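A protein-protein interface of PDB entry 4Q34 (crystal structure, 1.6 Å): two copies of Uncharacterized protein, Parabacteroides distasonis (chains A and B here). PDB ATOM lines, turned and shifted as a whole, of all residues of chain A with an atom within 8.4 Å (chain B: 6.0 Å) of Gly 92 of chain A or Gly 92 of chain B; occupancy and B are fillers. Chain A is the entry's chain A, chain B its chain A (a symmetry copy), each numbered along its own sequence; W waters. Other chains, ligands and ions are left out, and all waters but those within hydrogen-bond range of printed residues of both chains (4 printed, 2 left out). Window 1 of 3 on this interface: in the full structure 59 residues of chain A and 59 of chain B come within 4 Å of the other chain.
The side-chain amide oxygen of Asn 93 of chain B lies close to the side-chain carboxylate of Asp 87 of chain A, 3.0 Å away.
The side-chain amide oxygen (OD1) of Asn 93 of chain A lies close to the side-chain carboxylate (OD2) of Asp 87 of chain B (3.0 Å).
The backbone NH of Asn 93 of chain A is in hydrogen-bond range of the side-chain amide oxygen of Asn 93 of chain B (3.1 Å).
The side-chain hydroxyl (OG1) of Thr 145 of chain B is in hydrogen-bond range of the backbone NH (N) of Gly 95 of chain A, 3.3 Å away.
The side-chain sulfur (SD) of Met 144 of chain A lies close to the guanidinium group (NH1) of Arg 96 of chain B.
N of Gly 95 of chain B is in hydrogen-bond range of OG1 of Thr 145 of chain A, 3.3 Å away.
The backbone carbonyl oxygen of Tyr 35 of chain A is in hydrogen-bond range of the backbone NH of Asp 87 of chain A (2.8 Å).
The backbone carbonyl oxygen of Gly 56 of chain A is in hydrogen-bond range of the backbone NH of Thr 145 of chain A, at 2.9 Å.
OD1 of Asp 87 of chain A lies within hydrogen-bond range of N of Ser 59 of chain A, at 2.9 Å.
The backbone carbonyl oxygen (O) of Arg 90 of chain A sits at hydrogen-bond distance from the backbone NH (N) of Ile 148 of chain A, at 2.7 Å.
Tyr 35 of chain A touches Phe 58 of chain B.
Gly 92 of chain A touches Asn 93 of chain B.
Gly 92 of chain A touches Thr 145 of chain B (O to OG1, 3.6 Å).
Phe 58 of chain B touches Asn 93 of chain A (CE2 to CG, 3.3 Å).
Gly 95 of chain A touches Pro 146 of chain B (C to CD, 3.5 Å).
Thr 145 of chain B touches Arg 96 of chain A.
Arg 96 of chain A touches Pro 146 of chain B.
Thr 145 of chain A touches Asn 93 of chain B.
Pro 146 of chain A touches Arg 96 of chain B (CD to N, 3.7 Å).
Ile 148 of chain A touches Ile 148 of chain B.
Of chain A, only Gly 92 (3.2 Å), Asn 93 (3.6 Å) and Thr 145 (3.6 Å) come within 4 Å of Gly 92 of chain B.
Printed residues of chain A within 4 Å of Phe 58 of chain B: Tyr 35 (3.6 Å) and Asn 93 (3.3 Å).
Of the printed residues of chain B, Met 144 of chain A touches Arg 96 (3.4 Å).
Of the printed residues of chain B, Phe 58 of chain A touches Asn 93.
Printed residues of chain B within 4 Å of Thr 145 of chain A: Gly 92 (3.6 Å), Asn 93 (3.6 Å), Gly 95 (3.3 Å) and Arg 96 (3.8 Å).
Of the printed residues of chain A, Arg 96 of chain B touches Met 144, Thr 145 and Pro 146.
Ser 59 of chain A touches none of the printed residues of chain B.
The nearest residue of chain B that does not touch Gly 92 of chain A is Arg 91 of chain B (5.5 Å).
The nearest residue of chain A that does not touch Gly 92 of chain B is Arg 91 of chain A (5.5 Å).
Of the 13 printed residues of chain B, 9 touch a printed residue of chain A.
Hydrophobic or aromatic side chains of chain B within 4 Å of the printed part of chain A: Phe 58, Pro 146 and Ile 148.
Printed residues of chain A that touch a printed residue of chain B: Tyr 35, Phe 58, Asp 87, Gly 92, Asn 93, Gly 95, Arg 96, Met 144, Thr 145, Pro 146 and Ile 148.
Among the printed residues, 23 pairs touch across the chains.
Phe 58 of chain A touches Asn 93 of chain B, and with the chains exchanged Asn 93 of chain A touches Phe 58 of chain B.
Asn 93 of chain A touches Thr 145 of chain B, and with the chains exchanged Thr 145 of chain A touches Asn 93 of chain B.
Gly 95 of chain A touches Pro 146 of chain B, and with the chains exchanged Pro 146 of chain A touches Gly 95 of chain B.
Ile 148 of chain A touches its own counterpart, Ile 148 of chain B.
Positions printed for both chains: 58, 87, 88, 90, 91, 92, 93, 94, 95, 96, 145, 146 and 148.
Water W1 lies within hydrogen-bond range of the side-chain hydroxyl of Ser 59 of chain A (2.7 Å), the side-chain carboxylate of Asp 87 of chain A (2.7 Å) and the side-chain amide nitrogen of Asn 93 of chain B (2.9 Å).
Water W4 lies within hydrogen-bond range of OD2 of Asp 87 of chain B (2.7 Å) and ND2 of Asn 93 of chain A (2.9 Å).
Water W2 lies within hydrogen-bond range of O of Gly 92 of chain B and O of Gly 92 of chain A.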
ATOM      1  N   HIS A  33     -11.591  17.659  20.419  1.00  0.00           N
ATOM      2  CA  HIS A  33     -10.432  18.413  20.916  1.00  0.00           C
ATOM      3  C   HIS A  33      -9.233  18.023  20.083  1.00  0.00           C
ATOM      4  O   HIS A  33      -9.227  16.986  19.382  1.00  0.00           O
ATOM      5  CB  HIS A  33     -10.162  18.047  22.377  1.00  0.00           C
ATOM      6  CG  HIS A  33     -10.163  16.565  22.600  1.00  0.00           C
ATOM      7  ND1 HIS A  33     -11.328  15.858  22.804  1.00  0.00           N
ATOM      8  CD2 HIS A  33      -9.170  15.636  22.531  1.00  0.00           C
ATOM      9  CE1 HIS A  33     -11.045  14.568  22.892  1.00  0.00           C
ATOM     10  NE2 HIS A  33      -9.744  14.411  22.735  1.00  0.00           N
ATOM     11  N   TYR A  35      -5.056  17.064  20.635  1.00  0.00           N
ATOM     12  CA  TYR A  35      -4.118  16.627  21.640  1.00  0.00           C
ATOM     13  C   TYR A  35      -2.799  17.353  21.400  1.00  0.00           C
ATOM     14  O   TYR A  35      -2.385  17.503  20.265  1.00  0.00           O
ATOM     15  CB  TYR A  35      -3.887  15.126  21.604  1.00  0.00           C
ATOM     16  CG  TYR A  35      -2.649  14.668  22.365  1.00  0.00           C
ATOM     17  CD1 TYR A  35      -1.441  14.575  21.727  1.00  0.00           C
ATOM     18  CD2 TYR A  35      -2.709  14.311  23.700  1.00  0.00           C
ATOM     19  CE1 TYR A  35      -0.298  14.133  22.391  1.00  0.00           C
ATOM     20  CE2 TYR A  35      -1.577  13.872  24.390  1.00  0.00           C
ATOM     21  CZ  TYR A  35      -0.366  13.773  23.719  1.00  0.00           C
ATOM     22  OH  TYR A  35       0.776  13.354  24.363  1.00  0.00           O
ATOM     23  N   HIS A  53       0.169  19.241  11.304  1.00  0.00           N
ATOM     24  CA  HIS A  53       0.306  18.232  10.251  1.00  0.00           C
ATOM     25  C   HIS A  53      -0.806  18.341   9.198  1.00  0.00           C
ATOM     26  O   HIS A  53      -1.788  19.102   9.359  1.00  0.00           O
ATOM     27  CB  HIS A  53       0.247  16.857  10.913  1.00  0.00           C
ATOM     28  CG  HIS A  53      -1.048  16.599  11.611  1.00  0.00           C
ATOM     29  ND1 HIS A  53      -2.184  16.244  10.927  1.00  0.00           N
ATOM     30  CD2 HIS A  53      -1.422  16.737  12.906  1.00  0.00           C
ATOM     31  CE1 HIS A  53      -3.185  16.114  11.774  1.00  0.00           C
ATOM     32  NE2 HIS A  53      -2.750  16.411  12.980  1.00  0.00           N
ATOM     33  N   GLY A  56      -3.951  12.450   6.792  1.00  0.00           N
ATOM     34  CA  GLY A  56      -3.432  11.090   7.004  1.00  0.00           C
ATOM     35  C   GLY A  56      -2.244  10.972   7.951  1.00  0.00           C
ATOM     36  O   GLY A  56      -1.740   9.877   8.128  1.00  0.00           O
ATOM     37  N   GLN A  57      -1.802  12.084   8.564  1.00  0.00           N
ATOM     38  CA  GLN A  57      -0.570  12.151   9.344  1.00  0.00           C
ATOM     39  C   GLN A  57      -0.928  12.636  10.745  1.00  0.00           C
ATOM     40  O   GLN A  57      -2.085  13.033  11.015  1.00  0.00           O
ATOM     41  CB  GLN A  57       0.391  13.144   8.702  1.00  0.00           C
ATOM     42  CG  GLN A  57       0.848  12.748   7.284  1.00  0.00           C
ATOM     43  CD  GLN A  57       1.922  11.666   7.259  1.00  0.00           C
ATOM     44  OE1 GLN A  57       2.874  11.684   8.049  1.00  0.00           O
ATOM     45  NE2 GLN A  57       1.829  10.775   6.279  1.00  0.00           N
ATOM     46  N   PHE A  58       0.085  12.698  11.587  1.00  0.00           N
ATOM     47  CA  PHE A  58      -0.110  13.236  12.942  1.00  0.00           C
ATOM     48  C   PHE A  58       1.149  13.982  13.344  1.00  0.00           C
ATOM     49  O   PHE A  58       1.927  14.436  12.484  1.00  0.00           O
ATOM     50  CB  PHE A  58      -0.614  12.136  13.920  1.00  0.00           C
ATOM     51  CG  PHE A  58       0.352  11.009  14.182  1.00  0.00           C
ATOM     52  CD1 PHE A  58       0.496   9.939  13.288  1.00  0.00           C
ATOM     53  CD2 PHE A  58       1.163  10.993  15.348  1.00  0.00           C
ATOM     54  CE1 PHE A  58       1.362   8.869  13.555  1.00  0.00           C
ATOM     55  CE2 PHE A  58       2.029   9.928  15.582  1.00  0.00           C
ATOM     56  CZ  PHE A  58       2.186   8.901  14.668  1.00  0.00           C
ATOM     57  N   SER A  59       1.320  14.185  14.643  1.00  0.00           N
ATOM     58  CA  SER A  59       2.473  14.914  15.134  1.00  0.00           C
ATOM     59  C   SER A  59       3.801  14.342  14.649  1.00  0.00           C
ATOM     60  O   SER A  59       4.781  15.082  14.605  1.00  0.00           O
ATOM     61  CB  SER A  59       2.448  14.915  16.664  1.00  0.00           C
ATOM     62  OG  SER A  59       2.528  13.611  17.189  1.00  0.00           O
ATOM     63  N   VAL A  86       1.024  18.891  17.754  1.00  0.00           N
ATOM     64  CA  VAL A  86      -0.407  18.714  17.879  1.00  0.00           C
ATOM     65  C   VAL A  86      -0.872  17.525  17.035  1.00  0.00           C
ATOM     66  O   VAL A  86      -0.364  17.323  15.912  1.00  0.00           O
ATOM     67  CB  VAL A  86      -1.146  20.020  17.436  1.00  0.00           C
ATOM     68  CG1 VAL A  86      -2.655  19.855  17.595  1.00  0.00           C
ATOM     69  CG2 VAL A  86      -0.612  21.256  18.208  1.00  0.00           C
ATOM     70  N   ASP A  87      -1.833  16.758  17.575  1.00  0.00           N
ATOM     71  CA  ASP A  87      -2.707  15.895  16.800  1.00  0.00           C
ATOM     72  C   ASP A  87      -4.076  16.605  16.767  1.00  0.00           C
ATOM     73  O   ASP A  87      -4.712  16.848  17.804  1.00  0.00           O
ATOM     74  CB  ASP A  87      -2.866  14.556  17.431  1.00  0.00           C
ATOM     75  CG  ASP A  87      -1.547  13.824  17.599  1.00  0.00           C
ATOM     76  OD1 ASP A  87      -0.639  13.876  16.739  1.00  0.00           O
ATOM     77  OD2 ASP A  87      -1.436  13.109  18.633  1.00  0.00           O
ATOM     78  N   GLN A  88      -4.472  17.010  15.570  1.00  0.00           N
ATOM     79  CA  GLN A  88      -5.653  17.789  15.373  1.00  0.00           C
ATOM     80  C   GLN A  88      -6.858  16.931  15.697  1.00  0.00           C
ATOM     81  O   GLN A  88      -6.743  15.719  15.786  1.00  0.00           O
ATOM     82  CB  GLN A  88      -5.708  18.343  13.938  1.00  0.00           C
ATOM     83  CG  GLN A  88      -6.270  17.361  12.921  1.00  0.00           C
ATOM     84  CD  GLN A  88      -6.138  17.753  11.473  1.00  0.00           C
ATOM     85  OE1 GLN A  88      -5.655  18.838  11.106  1.00  0.00           O
ATOM     86  NE2 GLN A  88      -6.594  16.831  10.601  1.00  0.00           N
ATOM     87  N   PRO A  89      -8.019  17.573  15.936  1.00  0.00           N
ATOM     88  CA  PRO A  89      -9.290  16.841  16.162  1.00  0.00           C
ATOM     89  C   PRO A  89      -9.458  15.669  15.205  1.00  0.00           C
ATOM     90  O   PRO A  89      -9.213  15.791  14.003  1.00  0.00           O
ATOM     91  CB  PRO A  89     -10.340  17.913  15.906  1.00  0.00           C
ATOM     92  CG  PRO A  89      -9.670  19.165  16.330  1.00  0.00           C
ATOM     93  CD  PRO A  89      -8.294  18.991  15.707  1.00  0.00           C
ATOM     94  N   ARG A  90      -9.920  14.557  15.771  1.00  0.00           N
ATOM     95  CA  ARG A  90     -10.255  13.319  15.044  1.00  0.00           C
ATOM     96  C   ARG A  90      -9.058  12.552  14.495  1.00  0.00           C
ATOM     97  O   ARG A  90      -9.231  11.695  13.663  1.00  0.00           O
ATOM     98  CB  ARG A  90     -11.248  13.607  13.913  1.00  0.00           C
ATOM     99  CG  ARG A  90     -12.452  14.380  14.395  1.00  0.00           C
ATOM    100  CD  ARG A  90     -13.337  14.887  13.254  1.00  0.00           C
ATOM    101  NE  ARG A  90     -14.497  15.579  13.812  1.00  0.00           N
ATOM    102  CZ  ARG A  90     -15.388  16.287  13.108  1.00  0.00           C
ATOM    103  NH1 ARG A  90     -15.266  16.411  11.782  1.00  0.00           N
ATOM    104  NH2 ARG A  90     -16.429  16.848  13.735  1.00  0.00           N
ATOM    105  N   ARG A  91      -7.855  12.883  14.955  1.00  0.00           N
ATOM    106  CA  ARG A  91      -6.629  12.288  14.448  1.00  0.00           C
ATOM    107  C   ARG A  91      -5.750  11.745  15.585  1.00  0.00           C
ATOM    108  O   ARG A  91      -5.434  12.455  16.578  1.00  0.00           O
ATOM    109  CB  ARG A  91      -5.855  13.312  13.644  1.00  0.00           C
ATOM    110  CG  ARG A  91      -4.764  12.728  12.775  1.00  0.00           C
ATOM    111  CD  ARG A  91      -5.287  11.931  11.575  1.00  0.00           C
ATOM    112  NE  ARG A  91      -6.072  12.712  10.619  1.00  0.00           N
ATOM    113  CZ  ARG A  91      -5.601  13.610   9.745  1.00  0.00           C
ATOM    114  NH1 ARG A  91      -4.302  13.962   9.696  1.00  0.00           N
ATOM    115  NH2 ARG A  91      -6.456  14.217   8.930  1.00  0.00           N
ATOM    116  N   GLY A  92      -5.295  10.514  15.445  1.00  0.00           N
ATOM    117  CA  GLY A  92      -4.305   9.941  16.386  1.00  0.00           C
ATOM    118  C   GLY A  92      -4.794   9.949  17.828  1.00  0.00           C
ATOM    119  O   GLY A  92      -5.873   9.478  18.083  1.00  0.00           O
ATOM    120  N   ASN A  93      -3.993  10.529  18.742  1.00  0.00           N
ATOM    121  CA  ASN A  93      -4.368  10.623  20.156  1.00  0.00           C
ATOM    122  C   ASN A  93      -5.633  11.461  20.397  1.00  0.00           C
ATOM    123  O   ASN A  93      -6.253  11.377  21.465  1.00  0.00           O
ATOM    124  CB  ASN A  93      -3.224  11.238  20.936  1.00  0.00           C
ATOM    125  CG  ASN A  93      -2.016  10.308  21.067  1.00  0.00           C
ATOM    126  OD1 ASN A  93      -2.092   9.112  20.840  1.00  0.00           O
ATOM    127  ND2 ASN A  93      -0.891  10.882  21.493  1.00  0.00           N
ATOM    128  N   ALA A  94      -5.991  12.276  19.402  1.00  0.00           N
ATOM    129  CA  ALA A  94      -7.258  13.036  19.438  1.00  0.00           C
ATOM    130  C   ALA A  94      -8.352  12.302  18.692  1.00  0.00           C
ATOM    131  O   ALA A  94      -9.214  12.929  18.113  1.00  0.00           O
ATOM    132  CB  ALA A  94      -7.054  14.425  18.869  1.00  0.00           C
ATOM    133  N   GLY A  95      -8.303  10.975  18.709  1.00  0.00           N
ATOM    134  CA  GLY A  95      -9.277  10.138  17.983  1.00  0.00           C
ATOM    135  C   GLY A  95     -10.693  10.163  18.470  1.00  0.00           C
ATOM    136  O   GLY A  95     -11.566   9.667  17.786  1.00  0.00           O
ATOM    137  N   ARG A  96     -10.940  10.732  19.644  1.00  0.00           N
ATOM    138  CA  ARG A  96     -12.285  10.813  20.233  1.00  0.00           C
ATOM    139  C   ARG A  96     -13.058  11.940  19.545  1.00  0.00           C
ATOM    140  O   ARG A  96     -13.194  13.045  20.085  1.00  0.00           O
ATOM    141  CB  ARG A  96     -12.202  11.038  21.749  1.00  0.00           C
ATOM    142  CG  ARG A  96     -13.554  10.975  22.464  1.00  0.00           C
ATOM    143  CD  ARG A  96     -13.298  11.005  23.926  1.00  0.00           C
ATOM    144  NE  ARG A  96     -14.514  10.919  24.777  1.00  0.00           N
ATOM    145  CZ  ARG A  96     -15.104   9.802  25.200  1.00  0.00           C
ATOM    146  NH1 ARG A  96     -14.710   8.602  24.809  1.00  0.00           N
ATOM    147  NH2 ARG A  96     -16.155   9.879  26.024  1.00  0.00           N
ATOM    148  N   GLY A  97     -13.543  11.647  18.338  1.00  0.00           N
ATOM    149  CA  GLY A  97     -14.388  12.581  17.581  1.00  0.00           C
ATOM    150  C   GLY A  97     -15.829  12.438  17.996  1.00  0.00           C
ATOM    151  O   GLY A  97     -16.173  11.540  18.746  1.00  0.00           O
ATOM    152  N   MET A 144       1.324   7.106   9.183  1.00  0.00           N
ATOM    153  CA  MET A 144      -0.023   7.480   8.789  1.00  0.00           C
ATOM    154  C   MET A 144      -0.982   6.985   9.845  1.00  0.00           C
ATOM    155  O   MET A 144      -0.742   5.956  10.500  1.00  0.00           O
ATOM    156  CB  MET A 144      -0.341   6.857   7.430  1.00  0.00           C
ATOM    157  CG  MET A 144       0.625   7.289   6.349  1.00  0.00           C
ATOM    158  SD  MET A 144       0.191   6.297   4.737  1.00  0.00           S
ATOM    159  CE  MET A 144       1.337   7.416   3.576  1.00  0.00           C
ATOM    160  N   THR A 145      -2.066   7.724  10.039  1.00  0.00           N
ATOM    161  CA  THR A 145      -3.131   7.342  10.982  1.00  0.00           C
ATOM    162  C   THR A 145      -4.443   7.919  10.424  1.00  0.00           C
ATOM    163  O   THR A 145      -4.423   8.967   9.802  1.00  0.00           O
ATOM    164  CB  THR A 145      -2.782   7.811  12.425  1.00  0.00           C
ATOM    165  OG1 THR A 145      -3.477   7.027  13.375  1.00  0.00           O
ATOM    166  CG2 THR A 145      -3.067   9.245  12.668  1.00  0.00           C
ATOM    167  N   PRO A 146      -5.599   7.252  10.662  1.00  0.00           N
ATOM    168  CA  PRO A 146      -6.841   7.657  10.039  1.00  0.00           C
ATOM    169  C   PRO A 146      -7.576   8.787  10.760  1.00  0.00           C
ATOM    170  O   PRO A 146      -7.300   9.078  11.924  1.00  0.00           O
ATOM    171  CB  PRO A 146      -7.661   6.364  10.024  1.00  0.00           C
ATOM    172  CG  PRO A 146      -7.167   5.642  11.262  1.00  0.00           C
ATOM    173  CD  PRO A 146      -5.711   5.929  11.313  1.00  0.00           C
ATOM    174  N   THR A 147      -8.457   9.457  10.033  1.00  0.00           N
ATOM    175  CA  THR A 147      -9.369  10.447  10.581  1.00  0.00           C
ATOM    176  C   THR A 147     -10.599   9.750  11.105  1.00  0.00           C
ATOM    177  O   THR A 147     -11.307   9.050  10.366  1.00  0.00           O
ATOM    178  CB  THR A 147      -9.725  11.476   9.500  1.00  0.00           C
ATOM    179  OG1 THR A 147      -8.512  12.148   9.096  1.00  0.00           O
ATOM    180  CG2 THR A 147     -10.762  12.472   9.964  1.00  0.00           C
ATOM    181  N   ILE A 148     -10.894   9.984  12.379  1.00  0.00           N
ATOM    182  CA  ILE A 148     -12.006   9.311  13.040  1.00  0.00           C
ATOM    183  C   ILE A 148     -13.230  10.220  12.954  1.00  0.00           C
ATOM    184  O   ILE A 148     -13.713  10.806  13.941  1.00  0.00           O
ATOM    185  CB  ILE A 148     -11.660   8.901  14.497  1.00  0.00           C
ATOM    186  CG1 ILE A 148     -10.246   8.283  14.590  1.00  0.00           C
ATOM    187  CG2 ILE A 148     -12.694   7.936  15.035  1.00  0.00           C
ATOM    188  CD1 ILE A 148      -9.959   7.177  13.592  1.00  0.00           C
ATOM    189  N   PHE B  58      -4.677   6.010  26.253  1.00  0.00           N
ATOM    190  CA  PHE B  58      -3.438   5.965  25.462  1.00  0.00           C
ATOM    191  C   PHE B  58      -2.281   6.358  26.363  1.00  0.00           C
ATOM    192  O   PHE B  58      -2.362   6.233  27.600  1.00  0.00           O
ATOM    193  CB  PHE B  58      -3.587   6.756  24.131  1.00  0.00           C
ATOM    194  CG  PHE B  58      -3.793   8.243  24.279  1.00  0.00           C
ATOM    195  CD1 PHE B  58      -5.050   8.787  24.572  1.00  0.00           C
ATOM    196  CD2 PHE B  58      -2.711   9.151  24.135  1.00  0.00           C
ATOM    197  CE1 PHE B  58      -5.249  10.171  24.665  1.00  0.00           C
ATOM    198  CE2 PHE B  58      -2.929  10.521  24.250  1.00  0.00           C
ATOM    199  CZ  PHE B  58      -4.170  11.038  24.579  1.00  0.00           C
ATOM    200  N   ASP B  87       1.507   3.962  22.568  1.00  0.00           N
ATOM    201  CA  ASP B  87       0.136   3.767  22.131  1.00  0.00           C
ATOM    202  C   ASP B  87       0.116   2.401  21.414  1.00  0.00           C
ATOM    203  O   ASP B  87       0.802   2.182  20.404  1.00  0.00           O
ATOM    204  CB  ASP B  87      -0.299   4.825  21.179  1.00  0.00           C
ATOM    205  CG  ASP B  87      -0.211   6.221  21.770  1.00  0.00           C
ATOM    206  OD1 ASP B  87      -0.501   6.460  22.964  1.00  0.00           O
ATOM    207  OD2 ASP B  87       0.116   7.142  20.972  1.00  0.00           O
ATOM    208  N   GLN B  88      -0.613   1.466  22.003  1.00  0.00           N
ATOM    209  CA  GLN B  88      -0.648   0.113  21.545  1.00  0.00           C
ATOM    210  C   GLN B  88      -1.338   0.077  20.197  1.00  0.00           C
ATOM    211  O   GLN B  88      -1.993   1.035  19.818  1.00  0.00           O
ATOM    212  CB  GLN B  88      -1.344  -0.795  22.574  1.00  0.00           C
ATOM    213  CG  GLN B  88      -2.861  -0.794  22.469  1.00  0.00           C
ATOM    214  CD  GLN B  88      -3.607  -1.475  23.586  1.00  0.00           C
ATOM    215  OE1 GLN B  88      -3.037  -2.064  24.521  1.00  0.00           O
ATOM    216  NE2 GLN B  88      -4.950  -1.401  23.487  1.00  0.00           N
ATOM    217  N   ARG B  90      -3.748  -0.130  17.170  1.00  0.00           N
ATOM    218  CA  ARG B  90      -5.145   0.291  16.962  1.00  0.00           C
ATOM    219  C   ARG B  90      -5.630   1.394  17.896  1.00  0.00           C
ATOM    220  O   ARG B  90      -6.813   1.612  17.996  1.00  0.00           O
ATOM    221  CB  ARG B  90      -6.092  -0.911  17.047  1.00  0.00           C
ATOM    222  CG  ARG B  90      -5.653  -2.045  16.152  1.00  0.00           C
ATOM    223  CD  ARG B  90      -6.435  -3.338  16.393  1.00  0.00           C
ATOM    224  NE  ARG B  90      -5.979  -4.362  15.455  1.00  0.00           N
ATOM    225  CZ  ARG B  90      -6.326  -5.654  15.491  1.00  0.00           C
ATOM    226  NH1 ARG B  90      -7.155  -6.111  16.436  1.00  0.00           N
ATOM    227  NH2 ARG B  90      -5.864  -6.488  14.552  1.00  0.00           N
ATOM    228  N   ARG B  91      -4.710   2.065  18.581  1.00  0.00           N
ATOM    229  CA  ARG B  91      -5.049   3.079  19.568  1.00  0.00           C
ATOM    230  C   ARG B  91      -4.294   4.392  19.312  1.00  0.00           C
ATOM    231  O   ARG B  91      -3.042   4.422  19.166  1.00  0.00           O
ATOM    232  CB  ARG B  91      -4.735   2.568  20.959  1.00  0.00           C
ATOM    233  CG  ARG B  91      -5.369   3.368  22.075  1.00  0.00           C
ATOM    234  CD  ARG B  91      -6.889   3.200  22.172  1.00  0.00           C
ATOM    235  NE  ARG B  91      -7.336   1.838  22.463  1.00  0.00           N
ATOM    236  CZ  ARG B  91      -7.248   1.204  23.638  1.00  0.00           C
ATOM    237  NH1 ARG B  91      -6.647   1.749  24.713  1.00  0.00           N
ATOM    238  NH2 ARG B  91      -7.725  -0.032  23.735  1.00  0.00           N
ATOM    239  N   GLY B  92      -5.015   5.498  19.309  1.00  0.00           N
ATOM    240  CA  GLY B  92      -4.383   6.836  19.243  1.00  0.00           C
ATOM    241  C   GLY B  92      -3.506   7.010  18.010  1.00  0.00           C
ATOM    242  O   GLY B  92      -3.964   6.757  16.926  1.00  0.00           O
ATOM    243  N   ASN B  93      -2.235   7.407  18.215  1.00  0.00           N
ATOM    244  CA  ASN B  93      -1.289   7.583  17.108  1.00  0.00           C
ATOM    245  C   ASN B  93      -1.002   6.284  16.341  1.00  0.00           C
ATOM    246  O   ASN B  93      -0.492   6.316  15.213  1.00  0.00           O
ATOM    247  CB  ASN B  93       0.018   8.124  17.652  1.00  0.00           C
ATOM    248  CG  ASN B  93      -0.080   9.577  18.120  1.00  0.00           C
ATOM    249  OD1 ASN B  93      -1.012  10.298  17.803  1.00  0.00           O
ATOM    250  ND2 ASN B  93       0.942  10.016  18.853  1.00  0.00           N
ATOM    251  N   ALA B  94      -1.318   5.151  16.971  1.00  0.00           N
ATOM    252  CA  ALA B  94      -1.226   3.837  16.301  1.00  0.00           C
ATOM    253  C   ALA B  94      -2.567   3.422  15.733  1.00  0.00           C
ATOM    254  O   ALA B  94      -2.866   2.247  15.686  1.00  0.00           O
ATOM    255  CB  ALA B  94      -0.701   2.791  17.264  1.00  0.00           C
ATOM    256  N   GLY B  95      -3.366   4.395  15.311  1.00  0.00           N
ATOM    257  CA  GLY B  95      -4.718   4.135  14.782  1.00  0.00           C
ATOM    258  C   GLY B  95      -4.810   3.399  13.482  1.00  0.00           C
ATOM    259  O   GLY B  95      -5.887   2.975  13.112  1.00  0.00           O
ATOM    260  N   ARG B  96      -3.698   3.238  12.774  1.00  0.00           N
ATOM    261  CA  ARG B  96      -3.659   2.541  11.480  1.00  0.00           C
ATOM    262  C   ARG B  96      -3.696   1.032  11.731  1.00  0.00           C
ATOM    263  O   ARG B  96      -2.667   0.349  11.674  1.00  0.00           O
ATOM    264  CB  ARG B  96      -2.412   2.944  10.682  1.00  0.00           C
ATOM    265  CG  ARG B  96      -2.375   2.386   9.257  1.00  0.00           C
ATOM    266  CD  ARG B  96      -1.232   3.016   8.550  1.00  0.00           C
ATOM    267  NE  ARG B  96      -1.069   2.606   7.131  1.00  0.00           N
ATOM    268  CZ  ARG B  96      -1.653   3.169   6.074  1.00  0.00           C
ATOM    269  NH1 ARG B  96      -2.553   4.129   6.192  1.00  0.00           N
ATOM    270  NH2 ARG B  96      -1.356   2.736   4.844  1.00  0.00           N
ATOM    271  N   THR B 145      -9.570   7.662  23.999  1.00  0.00           N
ATOM    272  CA  THR B 145      -9.479   7.585  22.531  1.00  0.00           C
ATOM    273  C   THR B 145      -9.938   6.172  22.133  1.00  0.00           C
ATOM    274  O   THR B 145      -9.722   5.235  22.882  1.00  0.00           O
ATOM    275  CB  THR B 145      -8.045   7.957  22.050  1.00  0.00           C
ATOM    276  OG1 THR B 145      -8.080   8.397  20.705  1.00  0.00           O
ATOM    277  CG2 THR B 145      -7.070   6.848  22.179  1.00  0.00           C
ATOM    278  N   PRO B 146     -10.556   6.003  20.937  1.00  0.00           N
ATOM    279  CA  PRO B 146     -11.146   4.733  20.571  1.00  0.00           C
ATOM    280  C   PRO B 146     -10.164   3.720  19.984  1.00  0.00           C
ATOM    281  O   PRO B 146      -9.065   4.078  19.562  1.00  0.00           O
ATOM    282  CB  PRO B 146     -12.227   5.130  19.561  1.00  0.00           C
ATOM    283  CG  PRO B 146     -11.635   6.365  18.909  1.00  0.00           C
ATOM    284  CD  PRO B 146     -10.952   7.086  20.012  1.00  0.00           C
ATOM    285  N   ILE B 148      -9.330   1.351  17.024  1.00  0.00           N
ATOM    286  CA  ILE B 148      -9.635   1.356  15.598  1.00  0.00           C
ATOM    287  C   ILE B 148      -9.523  -0.077  15.084  1.00  0.00           C
ATOM    288  O   ILE B 148      -8.609  -0.460  14.329  1.00  0.00           O
ATOM    289  CB  ILE B 148      -8.740   2.352  14.811  1.00  0.00           C
ATOM    290  CG1 ILE B 148      -8.605   3.700  15.554  1.00  0.00           C
ATOM    291  CG2 ILE B 148      -9.290   2.570  13.418  1.00  0.00           C
ATOM    292  CD1 ILE B 148      -9.914   4.324  16.001  1.00  0.00           C
HETATM  293  O   HOH W   1       1.182  12.839  19.400  1.00  0.00           O
HETATM  294  O   HOH W   2      -6.754   7.247  16.515  1.00  0.00           O
HETATM  295  O   HOH W   3      -0.874   4.662  12.988  1.00  0.00           O
HETATM  296  O   HOH W   4       1.335   9.222  22.277  1.00  0.00           O
